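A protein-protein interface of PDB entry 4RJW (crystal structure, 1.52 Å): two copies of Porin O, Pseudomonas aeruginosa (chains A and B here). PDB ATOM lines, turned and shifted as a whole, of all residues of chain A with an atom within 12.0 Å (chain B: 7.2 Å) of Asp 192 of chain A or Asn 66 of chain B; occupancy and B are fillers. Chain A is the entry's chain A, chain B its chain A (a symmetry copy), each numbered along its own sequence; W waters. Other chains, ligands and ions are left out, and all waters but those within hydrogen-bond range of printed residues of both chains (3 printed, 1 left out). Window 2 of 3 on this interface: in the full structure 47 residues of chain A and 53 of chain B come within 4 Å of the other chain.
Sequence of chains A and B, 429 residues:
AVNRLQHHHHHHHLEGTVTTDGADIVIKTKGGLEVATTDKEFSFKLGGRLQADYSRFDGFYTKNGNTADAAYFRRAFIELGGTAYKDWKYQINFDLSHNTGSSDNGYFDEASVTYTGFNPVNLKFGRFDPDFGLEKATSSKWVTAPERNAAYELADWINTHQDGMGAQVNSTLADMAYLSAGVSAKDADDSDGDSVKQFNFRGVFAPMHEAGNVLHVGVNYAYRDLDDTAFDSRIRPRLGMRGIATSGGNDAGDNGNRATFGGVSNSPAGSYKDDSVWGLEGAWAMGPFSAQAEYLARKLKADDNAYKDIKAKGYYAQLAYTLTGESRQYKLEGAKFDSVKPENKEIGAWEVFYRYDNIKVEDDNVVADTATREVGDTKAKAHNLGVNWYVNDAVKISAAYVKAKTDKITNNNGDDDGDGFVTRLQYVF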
ATOM      1  N   LYS A 186       8.954 -23.319 -11.023  1.00  0.00           N
ATOM      2  CA  LYS A 186      10.384 -23.054 -11.112  1.00  0.00           C
ATOM      3  C   LYS A 186      10.917 -22.612  -9.757  1.00  0.00           C
ATOM      4  O   LYS A 186      10.161 -22.100  -8.932  1.00  0.00           O
ATOM      5  CB  LYS A 186      10.648 -21.981 -12.170  1.00  0.00           C
ATOM      6  CG  LYS A 186      10.158 -22.345 -13.579  1.00  0.00           C
ATOM      7  CD  LYS A 186      10.608 -23.763 -13.994  1.00  0.00           C
ATOM      8  CE  LYS A 186      10.753 -23.925 -15.493  1.00  0.00           C
ATOM      9  NZ  LYS A 186      11.627 -22.877 -16.112  1.00  0.00           N
ATOM     10  N   ASP A 187      12.214 -22.802  -9.513  1.00  0.00           N
ATOM     11  CA  ASP A 187      12.728 -22.559  -8.157  1.00  0.00           C
ATOM     12  C   ASP A 187      13.005 -21.092  -7.811  1.00  0.00           C
ATOM     13  O   ASP A 187      14.158 -20.673  -7.627  1.00  0.00           O
ATOM     14  CB  ASP A 187      13.955 -23.426  -7.860  1.00  0.00           C
ATOM     15  CG  ASP A 187      14.366 -23.358  -6.399  1.00  0.00           C
ATOM     16  OD1 ASP A 187      13.480 -23.100  -5.556  1.00  0.00           O
ATOM     17  OD2 ASP A 187      15.567 -23.553  -6.106  1.00  0.00           O
ATOM     18  N   ALA A 188      11.924 -20.326  -7.698  1.00  0.00           N
ATOM     19  CA  ALA A 188      11.994 -18.959  -7.197  1.00  0.00           C
ATOM     20  C   ALA A 188      10.647 -18.655  -6.566  1.00  0.00           C
ATOM     21  O   ALA A 188       9.606 -18.993  -7.137  1.00  0.00           O
ATOM     22  CB  ALA A 188      12.272 -17.981  -8.333  1.00  0.00           C
ATOM     23  N   ASP A 189      10.661 -18.029  -5.395  1.00  0.00           N
ATOM     24  CA  ASP A 189       9.428 -17.758  -4.673  1.00  0.00           C
ATOM     25  C   ASP A 189       9.048 -16.293  -4.701  1.00  0.00           C
ATOM     26  O   ASP A 189       9.918 -15.422  -4.683  1.00  0.00           O
ATOM     27  CB  ASP A 189       9.564 -18.150  -3.197  1.00  0.00           C
ATOM     28  CG  ASP A 189       9.456 -19.640  -2.963  1.00  0.00           C
ATOM     29  OD1 ASP A 189       8.953 -20.372  -3.845  1.00  0.00           O
ATOM     30  OD2 ASP A 189       9.867 -20.068  -1.860  1.00  0.00           O
ATOM     31  N   ASP A 190       7.743 -16.029  -4.707  1.00  0.00           N
ATOM     32  CA  ASP A 190       7.242 -14.697  -4.377  1.00  0.00           C
ATOM     33  C   ASP A 190       7.350 -14.464  -2.864  1.00  0.00           C
ATOM     34  O   ASP A 190       7.884 -15.313  -2.135  1.00  0.00           O
ATOM     35  CB  ASP A 190       5.814 -14.480  -4.913  1.00  0.00           C
ATOM     36  CG  ASP A 190       4.772 -15.402  -4.275  1.00  0.00           C
ATOM     37  OD1 ASP A 190       4.994 -15.960  -3.176  1.00  0.00           O
ATOM     38  OD2 ASP A 190       3.683 -15.542  -4.873  1.00  0.00           O
ATOM     39  N   SER A 191       6.858 -13.330  -2.375  1.00  0.00           N
ATOM     40  CA  SER A 191       7.006 -13.037  -0.948  1.00  0.00           C
ATOM     41  C   SER A 191       6.185 -13.950  -0.040  1.00  0.00           C
ATOM     42  O   SER A 191       6.387 -13.966   1.176  1.00  0.00           O
ATOM     43  CB  SER A 191       6.713 -11.561  -0.650  1.00  0.00           C
ATOM     44  OG  SER A 191       5.330 -11.279  -0.717  1.00  0.00           O
ATOM     45  N   ASP A 192       5.265 -14.713  -0.624  1.00  0.00           N
ATOM     46  CA  ASP A 192       4.501 -15.690   0.151  1.00  0.00           C
ATOM     47  C   ASP A 192       5.110 -17.091   0.104  1.00  0.00           C
ATOM     48  O   ASP A 192       4.581 -18.001   0.732  1.00  0.00           O
ATOM     49  CB  ASP A 192       3.046 -15.764  -0.332  1.00  0.00           C
ATOM     50  CG  ASP A 192       2.245 -14.518   0.004  1.00  0.00           C
ATOM     51  OD1 ASP A 192       2.519 -13.861   1.040  1.00  0.00           O
ATOM     52  OD2 ASP A 192       1.320 -14.197  -0.775  1.00  0.00           O
ATOM     53  N   GLY A 193       6.203 -17.259  -0.639  1.00  0.00           N
ATOM     54  CA  GLY A 193       6.864 -18.554  -0.756  1.00  0.00           C
ATOM     55  C   GLY A 193       6.232 -19.427  -1.828  1.00  0.00           C
ATOM     56  O   GLY A 193       6.426 -20.647  -1.834  1.00  0.00           O
ATOM     57  N   ASP A 194       5.486 -18.804  -2.739  1.00  0.00           N
ATOM     58  CA  ASP A 194       4.826 -19.515  -3.841  1.00  0.00           C
ATOM     59  C   ASP A 194       5.714 -19.429  -5.088  1.00  0.00           C
ATOM     60  O   ASP A 194       6.137 -18.338  -5.484  1.00  0.00           O
ATOM     61  CB  ASP A 194       3.458 -18.866  -4.107  1.00  0.00           C
ATOM     62  CG  ASP A 194       2.458 -19.799  -4.768  1.00  0.00           C
ATOM     63  OD1 ASP A 194       2.782 -20.982  -4.995  1.00  0.00           O
ATOM     64  OD2 ASP A 194       1.320 -19.326  -5.022  1.00  0.00           O
ATOM     65  N   SER A 195       5.989 -20.572  -5.701  1.00  0.00           N
ATOM     66  CA  SER A 195       6.922 -20.654  -6.820  1.00  0.00           C
ATOM     67  C   SER A 195       6.422 -19.969  -8.090  1.00  0.00           C
ATOM     68  O   SER A 195       5.218 -19.838  -8.315  1.00  0.00           O
ATOM     69  CB  SER A 195       7.219 -22.118  -7.136  1.00  0.00           C
ATOM     70  OG  SER A 195       6.029 -22.776  -7.554  1.00  0.00           O
ATOM     71  N   VAL A 196       7.376 -19.538  -8.908  1.00  0.00           N
ATOM     72  CA  VAL A 196       7.090 -19.051 -10.249  1.00  0.00           C
ATOM     73  C   VAL A 196       6.469 -20.169 -11.077  1.00  0.00           C
ATOM     74  O   VAL A 196       7.027 -21.267 -11.166  1.00  0.00           O
ATOM     75  CB  VAL A 196       8.384 -18.558 -10.942  1.00  0.00           C
ATOM     76  CG1 VAL A 196       8.143 -18.331 -12.434  1.00  0.00           C
ATOM     77  CG2 VAL A 196       8.883 -17.273 -10.290  1.00  0.00           C
ATOM     78  N   LYS A 197       5.298 -19.900 -11.649  1.00  0.00           N
ATOM     79  CA  LYS A 197       4.642 -20.874 -12.516  1.00  0.00           C
ATOM     80  C   LYS A 197       4.855 -20.528 -13.983  1.00  0.00           C
ATOM     81  O   LYS A 197       4.841 -19.357 -14.374  1.00  0.00           O
ATOM     82  CB  LYS A 197       3.147 -20.947 -12.201  1.00  0.00           C
ATOM     83  CG  LYS A 197       2.830 -21.216 -10.728  1.00  0.00           C
ATOM     84  CD  LYS A 197       3.515 -22.482 -10.229  1.00  0.00           C
ATOM     85  CE  LYS A 197       3.012 -22.913  -8.851  1.00  0.00           C
ATOM     86  NZ  LYS A 197       3.172 -21.824  -7.850  1.00  0.00           N
ATOM     87  N   ASP A 225       4.913 -16.209 -14.791  1.00  0.00           N
ATOM     88  CA  ASP A 225       4.333 -15.172 -13.949  1.00  0.00           C
ATOM     89  C   ASP A 225       5.343 -14.797 -12.873  1.00  0.00           C
ATOM     90  O   ASP A 225       5.691 -15.623 -12.027  1.00  0.00           O
ATOM     91  CB  ASP A 225       3.052 -15.730 -13.309  1.00  0.00           C
ATOM     92  CG  ASP A 225       2.268 -14.685 -12.517  1.00  0.00           C
ATOM     93  OD1 ASP A 225       2.832 -13.640 -12.137  1.00  0.00           O
ATOM     94  OD2 ASP A 225       1.069 -14.929 -12.259  1.00  0.00           O
ATOM     95  N   LEU A 226       5.810 -13.549 -12.908  1.00  0.00           N
ATOM     96  CA  LEU A 226       6.840 -13.100 -11.977  1.00  0.00           C
ATOM     97  C   LEU A 226       6.297 -12.156 -10.909  1.00  0.00           C
ATOM     98  O   LEU A 226       7.074 -11.484 -10.229  1.00  0.00           O
ATOM     99  CB  LEU A 226       7.978 -12.407 -12.741  1.00  0.00           C
ATOM    100  CG  LEU A 226       8.740 -13.275 -13.752  1.00  0.00           C
ATOM    101  CD1 LEU A 226       9.675 -12.415 -14.576  1.00  0.00           C
ATOM    102  CD2 LEU A 226       9.532 -14.357 -13.039  1.00  0.00           C
ATOM    103  N   ASP A 227       4.977 -12.108 -10.752  1.00  0.00           N
ATOM    104  CA  ASP A 227       4.351 -11.225  -9.771  1.00  0.00           C
ATOM    105  C   ASP A 227       5.003 -11.349  -8.394  1.00  0.00           C
ATOM    106  O   ASP A 227       5.155 -12.460  -7.869  1.00  0.00           O
ATOM    107  CB  ASP A 227       2.856 -11.539  -9.664  1.00  0.00           C
ATOM    108  CG  ASP A 227       2.169 -10.735  -8.580  1.00  0.00           C
ATOM    109  OD1 ASP A 227       2.271  -9.491  -8.596  1.00  0.00           O
ATOM    110  OD2 ASP A 227       1.540 -11.359  -7.699  1.00  0.00           O
ATOM    111  N   ASP A 228       5.415 -10.209  -7.837  1.00  0.00           N
ATOM    112  CA  ASP A 228       5.919 -10.152  -6.464  1.00  0.00           C
ATOM    113  C   ASP A 228       7.111 -11.082  -6.239  1.00  0.00           C
ATOM    114  O   ASP A 228       7.283 -11.638  -5.160  1.00  0.00           O
ATOM    115  CB  ASP A 228       4.772 -10.464  -5.484  1.00  0.00           C
ATOM    116  CG  ASP A 228       5.165 -10.282  -4.032  1.00  0.00           C
ATOM    117  OD1 ASP A 228       5.801  -9.259  -3.712  1.00  0.00           O
ATOM    118  OD2 ASP A 228       4.853 -11.185  -3.220  1.00  0.00           O
ATOM    119  N   THR A 229       7.940 -11.249  -7.266  1.00  0.00           N
ATOM    120  CA  THR A 229       9.052 -12.190  -7.195  1.00  0.00           C
ATOM    121  C   THR A 229      10.380 -11.512  -7.513  1.00  0.00           C
ATOM    122  O   THR A 229      10.546 -10.920  -8.581  1.00  0.00           O
ATOM    123  CB  THR A 229       8.849 -13.387  -8.164  1.00  0.00           C
ATOM    124  OG1 THR A 229       7.608 -14.033  -7.867  1.00  0.00           O
ATOM    125  CG2 THR A 229       9.970 -14.402  -8.003  1.00  0.00           C
ATOM    126  N   ALA A 230      11.325 -11.598  -6.581  1.00  0.00           N
ATOM    127  CA  ALA A 230      12.680 -11.144  -6.859  1.00  0.00           C
ATOM    128  C   ALA A 230      13.382 -12.165  -7.743  1.00  0.00           C
ATOM    129  O   ALA A 230      13.258 -13.376  -7.527  1.00  0.00           O
ATOM    130  CB  ALA A 230      13.458 -10.906  -5.559  1.00  0.00           C
ATOM    131  N   PRO A 268      14.027  -6.530  -7.961  1.00  0.00           N
ATOM    132  CA  PRO A 268      13.226  -6.689  -6.741  1.00  0.00           C
ATOM    133  C   PRO A 268      11.827  -7.232  -6.984  1.00  0.00           C
ATOM    134  O   PRO A 268      11.275  -7.064  -8.071  1.00  0.00           O
ATOM    135  CB  PRO A 268      13.109  -5.255  -6.202  1.00  0.00           C
ATOM    136  CG  PRO A 268      14.168  -4.480  -6.894  1.00  0.00           C
ATOM    137  CD  PRO A 268      14.370  -5.121  -8.223  1.00  0.00           C
ATOM    138  N   ALA A 269      11.266  -7.880  -5.966  1.00  0.00           N
ATOM    139  CA  ALA A 269       9.863  -8.271  -6.002  1.00  0.00           C
ATOM    140  C   ALA A 269       9.012  -7.068  -6.388  1.00  0.00           C
ATOM    141  O   ALA A 269       9.145  -5.988  -5.805  1.00  0.00           O
ATOM    142  CB  ALA A 269       9.421  -8.818  -4.651  1.00  0.00           C
ATOM    143  N   GLY A 270       8.164  -7.249  -7.398  1.00  0.00           N
ATOM    144  CA  GLY A 270       7.261  -6.198  -7.818  1.00  0.00           C
ATOM    145  C   GLY A 270       7.769  -5.435  -9.026  1.00  0.00           C
ATOM    146  O   GLY A 270       7.042  -4.610  -9.583  1.00  0.00           O
ATOM    147  N   PHE B  57       0.419 -24.877   1.431  1.00  0.00           N
ATOM    148  CA  PHE B  57       0.188 -24.828   2.862  1.00  0.00           C
ATOM    149  C   PHE B  57       0.166 -23.379   3.332  1.00  0.00           C
ATOM    150  O   PHE B  57       0.750 -22.500   2.700  1.00  0.00           O
ATOM    151  CB  PHE B  57       1.271 -25.637   3.582  1.00  0.00           C
ATOM    152  CG  PHE B  57       2.642 -25.434   3.017  1.00  0.00           C
ATOM    153  CD1 PHE B  57       3.446 -24.410   3.489  1.00  0.00           C
ATOM    154  CD2 PHE B  57       3.120 -26.242   1.994  1.00  0.00           C
ATOM    155  CE1 PHE B  57       4.706 -24.210   2.964  1.00  0.00           C
ATOM    156  CE2 PHE B  57       4.378 -26.042   1.454  1.00  0.00           C
ATOM    157  CZ  PHE B  57       5.175 -25.031   1.943  1.00  0.00           C
ATOM    158  N   ASP B  58      -0.527 -23.144   4.441  1.00  0.00           N
ATOM    159  CA  ASP B  58      -0.694 -21.795   4.963  1.00  0.00           C
ATOM    160  C   ASP B  58      -0.840 -21.781   6.482  1.00  0.00           C
ATOM    161  O   ASP B  58      -0.555 -22.778   7.159  1.00  0.00           O
ATOM    162  CB  ASP B  58      -1.875 -21.104   4.267  1.00  0.00           C
ATOM    163  CG  ASP B  58      -3.223 -21.633   4.707  1.00  0.00           C
ATOM    164  OD1 ASP B  58      -3.294 -22.649   5.436  1.00  0.00           O
ATOM    165  OD2 ASP B  58      -4.250 -21.020   4.326  1.00  0.00           O
ATOM    166  N   GLY B  59      -1.268 -20.645   7.026  1.00  0.00           N
ATOM    167  CA  GLY B  59      -1.384 -20.523   8.466  1.00  0.00           C
ATOM    168  C   GLY B  59      -0.031 -20.689   9.136  1.00  0.00           C
ATOM    169  O   GLY B  59       0.977 -20.175   8.650  1.00  0.00           O
ATOM    170  N   TYR B  61       2.090 -22.867   9.105  1.00  0.00           N
ATOM    171  CA  TYR B  61       3.160 -23.429   8.284  1.00  0.00           C
ATOM    172  C   TYR B  61       4.010 -22.363   7.594  1.00  0.00           C
ATOM    173  O   TYR B  61       5.126 -22.647   7.159  1.00  0.00           O
ATOM    174  CB  TYR B  61       2.599 -24.409   7.244  1.00  0.00           C
ATOM    175  CG  TYR B  61       2.103 -25.704   7.837  1.00  0.00           C
ATOM    176  CD1 TYR B  61       2.981 -26.598   8.437  1.00  0.00           C
ATOM    177  CD2 TYR B  61       0.764 -26.032   7.783  1.00  0.00           C
ATOM    178  CE1 TYR B  61       2.530 -27.788   8.975  1.00  0.00           C
ATOM    179  CE2 TYR B  61       0.298 -27.214   8.317  1.00  0.00           C
ATOM    180  CZ  TYR B  61       1.190 -28.090   8.917  1.00  0.00           C
ATOM    181  OH  TYR B  61       0.736 -29.277   9.449  1.00  0.00           O
ATOM    182  N   THR B  62       3.489 -21.141   7.487  1.00  0.00           N
ATOM    183  CA  THR B  62       4.253 -20.066   6.865  1.00  0.00           C
ATOM    184  C   THR B  62       4.407 -18.889   7.828  1.00  0.00           C
ATOM    185  O   THR B  62       3.649 -18.771   8.791  1.00  0.00           O
ATOM    186  CB  THR B  62       3.619 -19.580   5.532  1.00  0.00           C
ATOM    187  OG1 THR B  62       2.387 -18.900   5.805  1.00  0.00           O
ATOM    188  CG2 THR B  62       3.376 -20.769   4.581  1.00  0.00           C
ATOM    189  N   LYS B  63       5.409 -18.049   7.593  1.00  0.00           N
ATOM    190  CA  LYS B  63       5.654 -16.947   8.515  1.00  0.00           C
ATOM    191  C   LYS B  63       4.533 -15.914   8.494  1.00  0.00           C
ATOM    192  O   LYS B  63       4.099 -15.449   9.548  1.00  0.00           O
ATOM    193  CB  LYS B  63       6.994 -16.273   8.229  1.00  0.00           C
ATOM    194  CG  LYS B  63       8.192 -17.153   8.575  1.00  0.00           C
ATOM    195  CD  LYS B  63       9.490 -16.414   8.343  1.00  0.00           C
ATOM    196  CE  LYS B  63      10.692 -17.339   8.462  1.00  0.00           C
ATOM    197  NZ  LYS B  63      11.942 -16.704   7.945  1.00  0.00           N
ATOM    198  N   ASN B  64       4.045 -15.567   7.305  1.00  0.00           N
ATOM    199  CA  ASN B  64       2.986 -14.560   7.229  1.00  0.00           C
ATOM    200  C   ASN B  64       1.572 -15.137   7.207  1.00  0.00           C
ATOM    201  O   ASN B  64       0.593 -14.390   7.222  1.00  0.00           O
ATOM    202  CB  ASN B  64       3.202 -13.568   6.071  1.00  0.00           C
ATOM    203  CG  ASN B  64       3.105 -14.220   4.699  1.00  0.00           C
ATOM    204  OD1 ASN B  64       2.577 -15.326   4.543  1.00  0.00           O
ATOM    205  ND2 ASN B  64       3.611 -13.522   3.694  1.00  0.00           N
ATOM    206  N   GLY B  65       1.469 -16.468   7.151  1.00  0.00           N
ATOM    207  CA  GLY B  65       0.176 -17.143   7.170  1.00  0.00           C
ATOM    208  C   GLY B  65      -0.437 -17.358   5.795  1.00  0.00           C
ATOM    209  O   GLY B  65      -1.394 -18.118   5.642  1.00  0.00           O
ATOM    210  N   ASN B  66       0.112 -16.689   4.784  1.00  0.00           N
ATOM    211  CA  ASN B  66      -0.398 -16.849   3.427  1.00  0.00           C
ATOM    212  C   ASN B  66       0.053 -18.184   2.844  1.00  0.00           C
ATOM    213  O   ASN B  66       0.917 -18.855   3.401  1.00  0.00           O
ATOM    214  CB  ASN B  66       0.046 -15.686   2.538  1.00  0.00           C
ATOM    215  CG  ASN B  66      -0.551 -14.367   2.974  1.00  0.00           C
ATOM    216  OD1 ASN B  66      -1.626 -14.328   3.584  1.00  0.00           O
ATOM    217  ND2 ASN B  66       0.135 -13.278   2.657  1.00  0.00           N
ATOM    218  N   THR B  67      -0.520 -18.565   1.711  1.00  0.00           N
ATOM    219  CA  THR B  67      -0.196 -19.858   1.104  1.00  0.00           C
ATOM    220  C   THR B  67       1.155 -19.868   0.393  1.00  0.00           C
ATOM    221  O   THR B  67       1.427 -19.037  -0.473  1.00  0.00           O
ATOM    222  CB  THR B  67      -1.296 -20.272   0.114  1.00  0.00           C
ATOM    223  OG1 THR B  67      -2.549 -20.368   0.810  1.00  0.00           O
ATOM    224  CG2 THR B  67      -0.974 -21.623  -0.541  1.00  0.00           C
ATOM    225  N   ALA B  68       2.006 -20.809   0.789  1.00  0.00           N
ATOM    226  CA  ALA B  68       3.260 -21.069   0.104  1.00  0.00           C
ATOM    227  C   ALA B  68       3.133 -22.405  -0.608  1.00  0.00           C
ATOM    228  O   ALA B  68       2.166 -23.143  -0.389  1.00  0.00           O
ATOM    229  CB  ALA B  68       4.401 -21.124   1.099  1.00  0.00           C
ATOM    230  N   ASP B  69       4.103 -22.714  -1.458  1.00  0.00           N
ATOM    231  CA  ASP B  69       4.148 -24.037  -2.056  1.00  0.00           C
ATOM    232  C   ASP B  69       5.544 -24.635  -2.042  1.00  0.00           C
ATOM    233  O   ASP B  69       6.518 -24.009  -1.611  1.00  0.00           O
ATOM    234  CB  ASP B  69       3.512 -24.061  -3.468  1.00  0.00           C
ATOM    235  CG  ASP B  69       4.421 -23.494  -4.560  1.00  0.00           C
ATOM    236  OD1 ASP B  69       5.462 -22.864  -4.258  1.00  0.00           O
ATOM    237  OD2 ASP B  69       4.072 -23.665  -5.744  1.00  0.00           O
ATOM    238  N   ASP B 251      10.994 -24.803  -2.234  1.00  0.00           N
ATOM    239  CA  ASP B 251      10.253 -24.852  -0.981  1.00  0.00           C
ATOM    240  C   ASP B 251       9.640 -23.478  -0.683  1.00  0.00           C
ATOM    241  O   ASP B 251       9.559 -22.624  -1.574  1.00  0.00           O
ATOM    242  CB  ASP B 251      11.119 -25.395   0.182  1.00  0.00           C
ATOM    243  CG  ASP B 251      12.240 -24.450   0.607  1.00  0.00           C
ATOM    244  OD1 ASP B 251      12.333 -23.299   0.115  1.00  0.00           O
ATOM    245  OD2 ASP B 251      13.038 -24.860   1.480  1.00  0.00           O
ATOM    246  N   ALA B 252       9.199 -23.275   0.554  1.00  0.00           N
ATOM    247  CA  ALA B 252       8.521 -22.040   0.950  1.00  0.00           C
ATOM    248  C   ALA B 252       9.479 -20.870   1.128  1.00  0.00           C
ATOM    249  O   ALA B 252       9.041 -19.748   1.394  1.00  0.00           O
ATOM    250  CB  ALA B 252       7.724 -22.267   2.230  1.00  0.00           C
ATOM    251  N   GLY B 253      10.774 -21.133   0.988  1.00  0.00           N
ATOM    252  CA  GLY B 253      11.777 -20.083   1.086  1.00  0.00           C
ATOM    253  C   GLY B 253      11.683 -19.285   2.367  1.00  0.00           C
ATOM    254  O   GLY B 253      11.464 -19.828   3.453  1.00  0.00           O
ATOM    255  N   ASP B 254      11.827 -17.970   2.225  1.00  0.00           N
ATOM    256  CA  ASP B 254      11.815 -17.070   3.365  1.00  0.00           C
ATOM    257  C   ASP B 254      10.480 -17.012   4.096  1.00  0.00           C
ATOM    258  O   ASP B 254      10.414 -16.491   5.209  1.00  0.00           O
ATOM    259  CB  ASP B 254      12.231 -15.669   2.924  1.00  0.00           C
ATOM    260  CG  ASP B 254      13.703 -15.586   2.551  1.00  0.00           C
ATOM    261  OD1 ASP B 254      14.484 -16.472   2.967  1.00  0.00           O
ATOM    262  OD2 ASP B 254      14.082 -14.628   1.843  1.00  0.00           O
ATOM    263  N   ASN B 255       9.422 -17.541   3.491  1.00  0.00           N
ATOM    264  CA  ASN B 255       8.129 -17.545   4.152  1.00  0.00           C
ATOM    265  C   ASN B 255       7.790 -18.902   4.771  1.00  0.00           C
ATOM    266  O   ASN B 255       6.696 -19.082   5.291  1.00  0.00           O
ATOM    267  CB  ASN B 255       7.008 -17.121   3.202  1.00  0.00           C
ATOM    268  CG  ASN B 255       5.751 -16.678   3.945  1.00  0.00           C
ATOM    269  OD1 ASN B 255       5.823 -16.040   5.006  1.00  0.00           O
ATOM    270  ND2 ASN B 255       4.582 -17.016   3.384  1.00  0.00           N
ATOM    271  N   GLY B 256       8.717 -19.851   4.736  1.00  0.00           N
ATOM    272  CA  GLY B 256       8.489 -21.105   5.446  1.00  0.00           C
ATOM    273  C   GLY B 256       8.663 -20.928   6.949  1.00  0.00           C
ATOM    274  O   GLY B 256       9.603 -20.265   7.384  1.00  0.00           O
ATOM    275  N   ASN B 411       2.946 -18.003  14.237  1.00  0.00           N
ATOM    276  CA  ASN B 411       3.780 -17.349  13.241  1.00  0.00           C
ATOM    277  C   ASN B 411       3.717 -15.828  13.418  1.00  0.00           C
ATOM    278  O   ASN B 411       3.171 -15.321  14.408  1.00  0.00           O
ATOM    279  CB  ASN B 411       3.380 -17.747  11.820  1.00  0.00           C
ATOM    280  CG  ASN B 411       1.940 -17.386  11.491  1.00  0.00           C
ATOM    281  OD1 ASN B 411       1.300 -16.607  12.204  1.00  0.00           O
ATOM    282  ND2 ASN B 411       1.432 -17.929  10.393  1.00  0.00           N
ATOM    283  N   ASN B 413       1.938 -13.838  11.847  1.00  0.00           N
ATOM    284  CA  ASN B 413       0.562 -13.398  11.651  1.00  0.00           C
ATOM    285  C   ASN B 413      -0.303 -13.659  12.884  1.00  0.00           C
ATOM    286  O   ASN B 413      -1.475 -13.275  12.919  1.00  0.00           O
ATOM    287  CB  ASN B 413      -0.033 -14.131  10.440  1.00  0.00           C
ATOM    288  CG  ASN B 413      -1.342 -13.521   9.959  1.00  0.00           C
ATOM    289  OD1 ASN B 413      -1.459 -12.301   9.799  1.00  0.00           O
ATOM    290  ND2 ASN B 413      -2.337 -14.375   9.717  1.00  0.00           N
ATOM    291  N   ASP B 415      -1.076 -16.743  13.806  1.00  0.00           N
ATOM    292  CA  ASP B 415      -1.799 -17.992  13.567  1.00  0.00           C
ATOM    293  C   ASP B 415      -1.377 -19.071  14.555  1.00  0.00           C
ATOM    294  O   ASP B 415      -0.177 -19.307  14.749  1.00  0.00           O
ATOM    295  CB  ASP B 415      -1.532 -18.506  12.151  1.00  0.00           C
ATOM    296  CG  ASP B 415      -2.059 -17.577  11.080  1.00  0.00           C
ATOM    297  OD1 ASP B 415      -3.194 -17.071  11.219  1.00  0.00           O
ATOM    298  OD2 ASP B 415      -1.343 -17.370  10.076  1.00  0.00           O
HETATM  299  O   HOH W   1      -0.115 -17.013  -1.558  1.00  0.00           O
HETATM  300  O   HOH W   2       3.111 -11.303   1.036  1.00  0.00           O
HETATM  301  O   HOH W   3      13.452 -22.956  -2.814  1.00  0.00           O
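O of Ser 191 of chain A touches ND2 of Asn 64 of chain B (3.8 Å). O of Ser 191 of chain A touches CB of Asn 255 of chain B, 3.8 Å away. Asp 192 of chain A touches Thr 67 of chain B. Gly 193 of chain A touches Asp 251 of chain B.
O of Asp 251 of chain B sits close to OD2 of Asp 189 of chain A (2.6 Å). The backbone NH of Gly 253 of chain B is in hydrogen-bond range of the side-chain carboxylate of Asp 189 of chain A (3.2 Å). The side-chain carboxylate (OD1) of Asp 192 of chain A sits at hydrogen-bond distance from the side-chain amide nitrogen (ND2) of Asn 64 of chain B, 2.9 Å away. ND2 of Asn 66 of chain B lies within hydrogen-bond range of OD1 of Asp 192 of chain A. The backbone carbonyl oxygen (O) of Asp 192 of chain A is in hydrogen-bond range of the side-chain amide nitrogen (ND2) of Asn 255 of chain B (2.8 Å). O of Gly 193 of chain A is in hydrogen-bond range of N of Asp 69 of chain B (3.1 Å). OD2 of Asp 69 of chain B lies within salt-bridge range of NZ of Lys 197 of chain A. The side-chain carboxylate (OD2) of Asp 189 of chain A sits close to the backbone carbonyl oxygen (O) of Ala 252 of chain B. The side-chain carboxylate of Asp 194 of chain A lies close to the side-chain carboxylate of Asp 69 of chain B.
No residue of chain A comes within 4 Å of Asp 58 of chain B. No residue of chain A comes within 4 Å of Gly 59 of chain B. No residue of chain A comes within 4 Å of Gly 65 of chain B. Thr 67 of chain B touches just one residue of chain A: Asp 192. Of the printed residues of chain B, Gly 193 of chain A touches Ala 68 (3.6 Å), Asp 69 (3.1 Å), Asp 251 (3.7 Å), Ala 252 (3.3 Å) and Asn 255 (3.9 Å). Of the printed residues of chain B, Ser 195 of chain A touches Asp 69 (2.8 Å). The nearest residue of chain B that does not touch Asp 192 of chain A is Ala 252 of chain B (4.8 Å). The nearest residue of chain A that does not touch Asn 66 of chain B is Ser 191 of chain A (6.5 Å).
Water W1 bridges the backbone carbonyl oxygen of Thr 67 of chain B (2.8 Å) and the side-chain carboxylate of Asp 192 of chain A (3.3 Å).
Printed residues of chain B that touch a printed residue of chain A: Asn 64, Asn 66, Thr 67, Ala 68, Asp 69, Asp 251, Ala 252, Gly 253 and Asn 255. Hydrophobic or aromatic side chains of chain B that line the printed part of chain A: Ala 68. Among the printed residues, 18 pairs touch across the chains. Among the printed residues, Asp or Glu carboxylates within 4 Å of a Lys or Arg side-chain nitrogen of the other chain: Lys 197 of chain A with Asp 69 of chain B (2.9 Å).
OD1 of Asp 194 of chain A is in salt-bridge range of NZ of Lys 197 of chain A, 3.0 Å away. The backbone NH of Asp 225 of chain A is in hydrogen-bond range of the backbone carbonyl oxygen of Lys 197 of chain A.
No position is printed for both chains.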
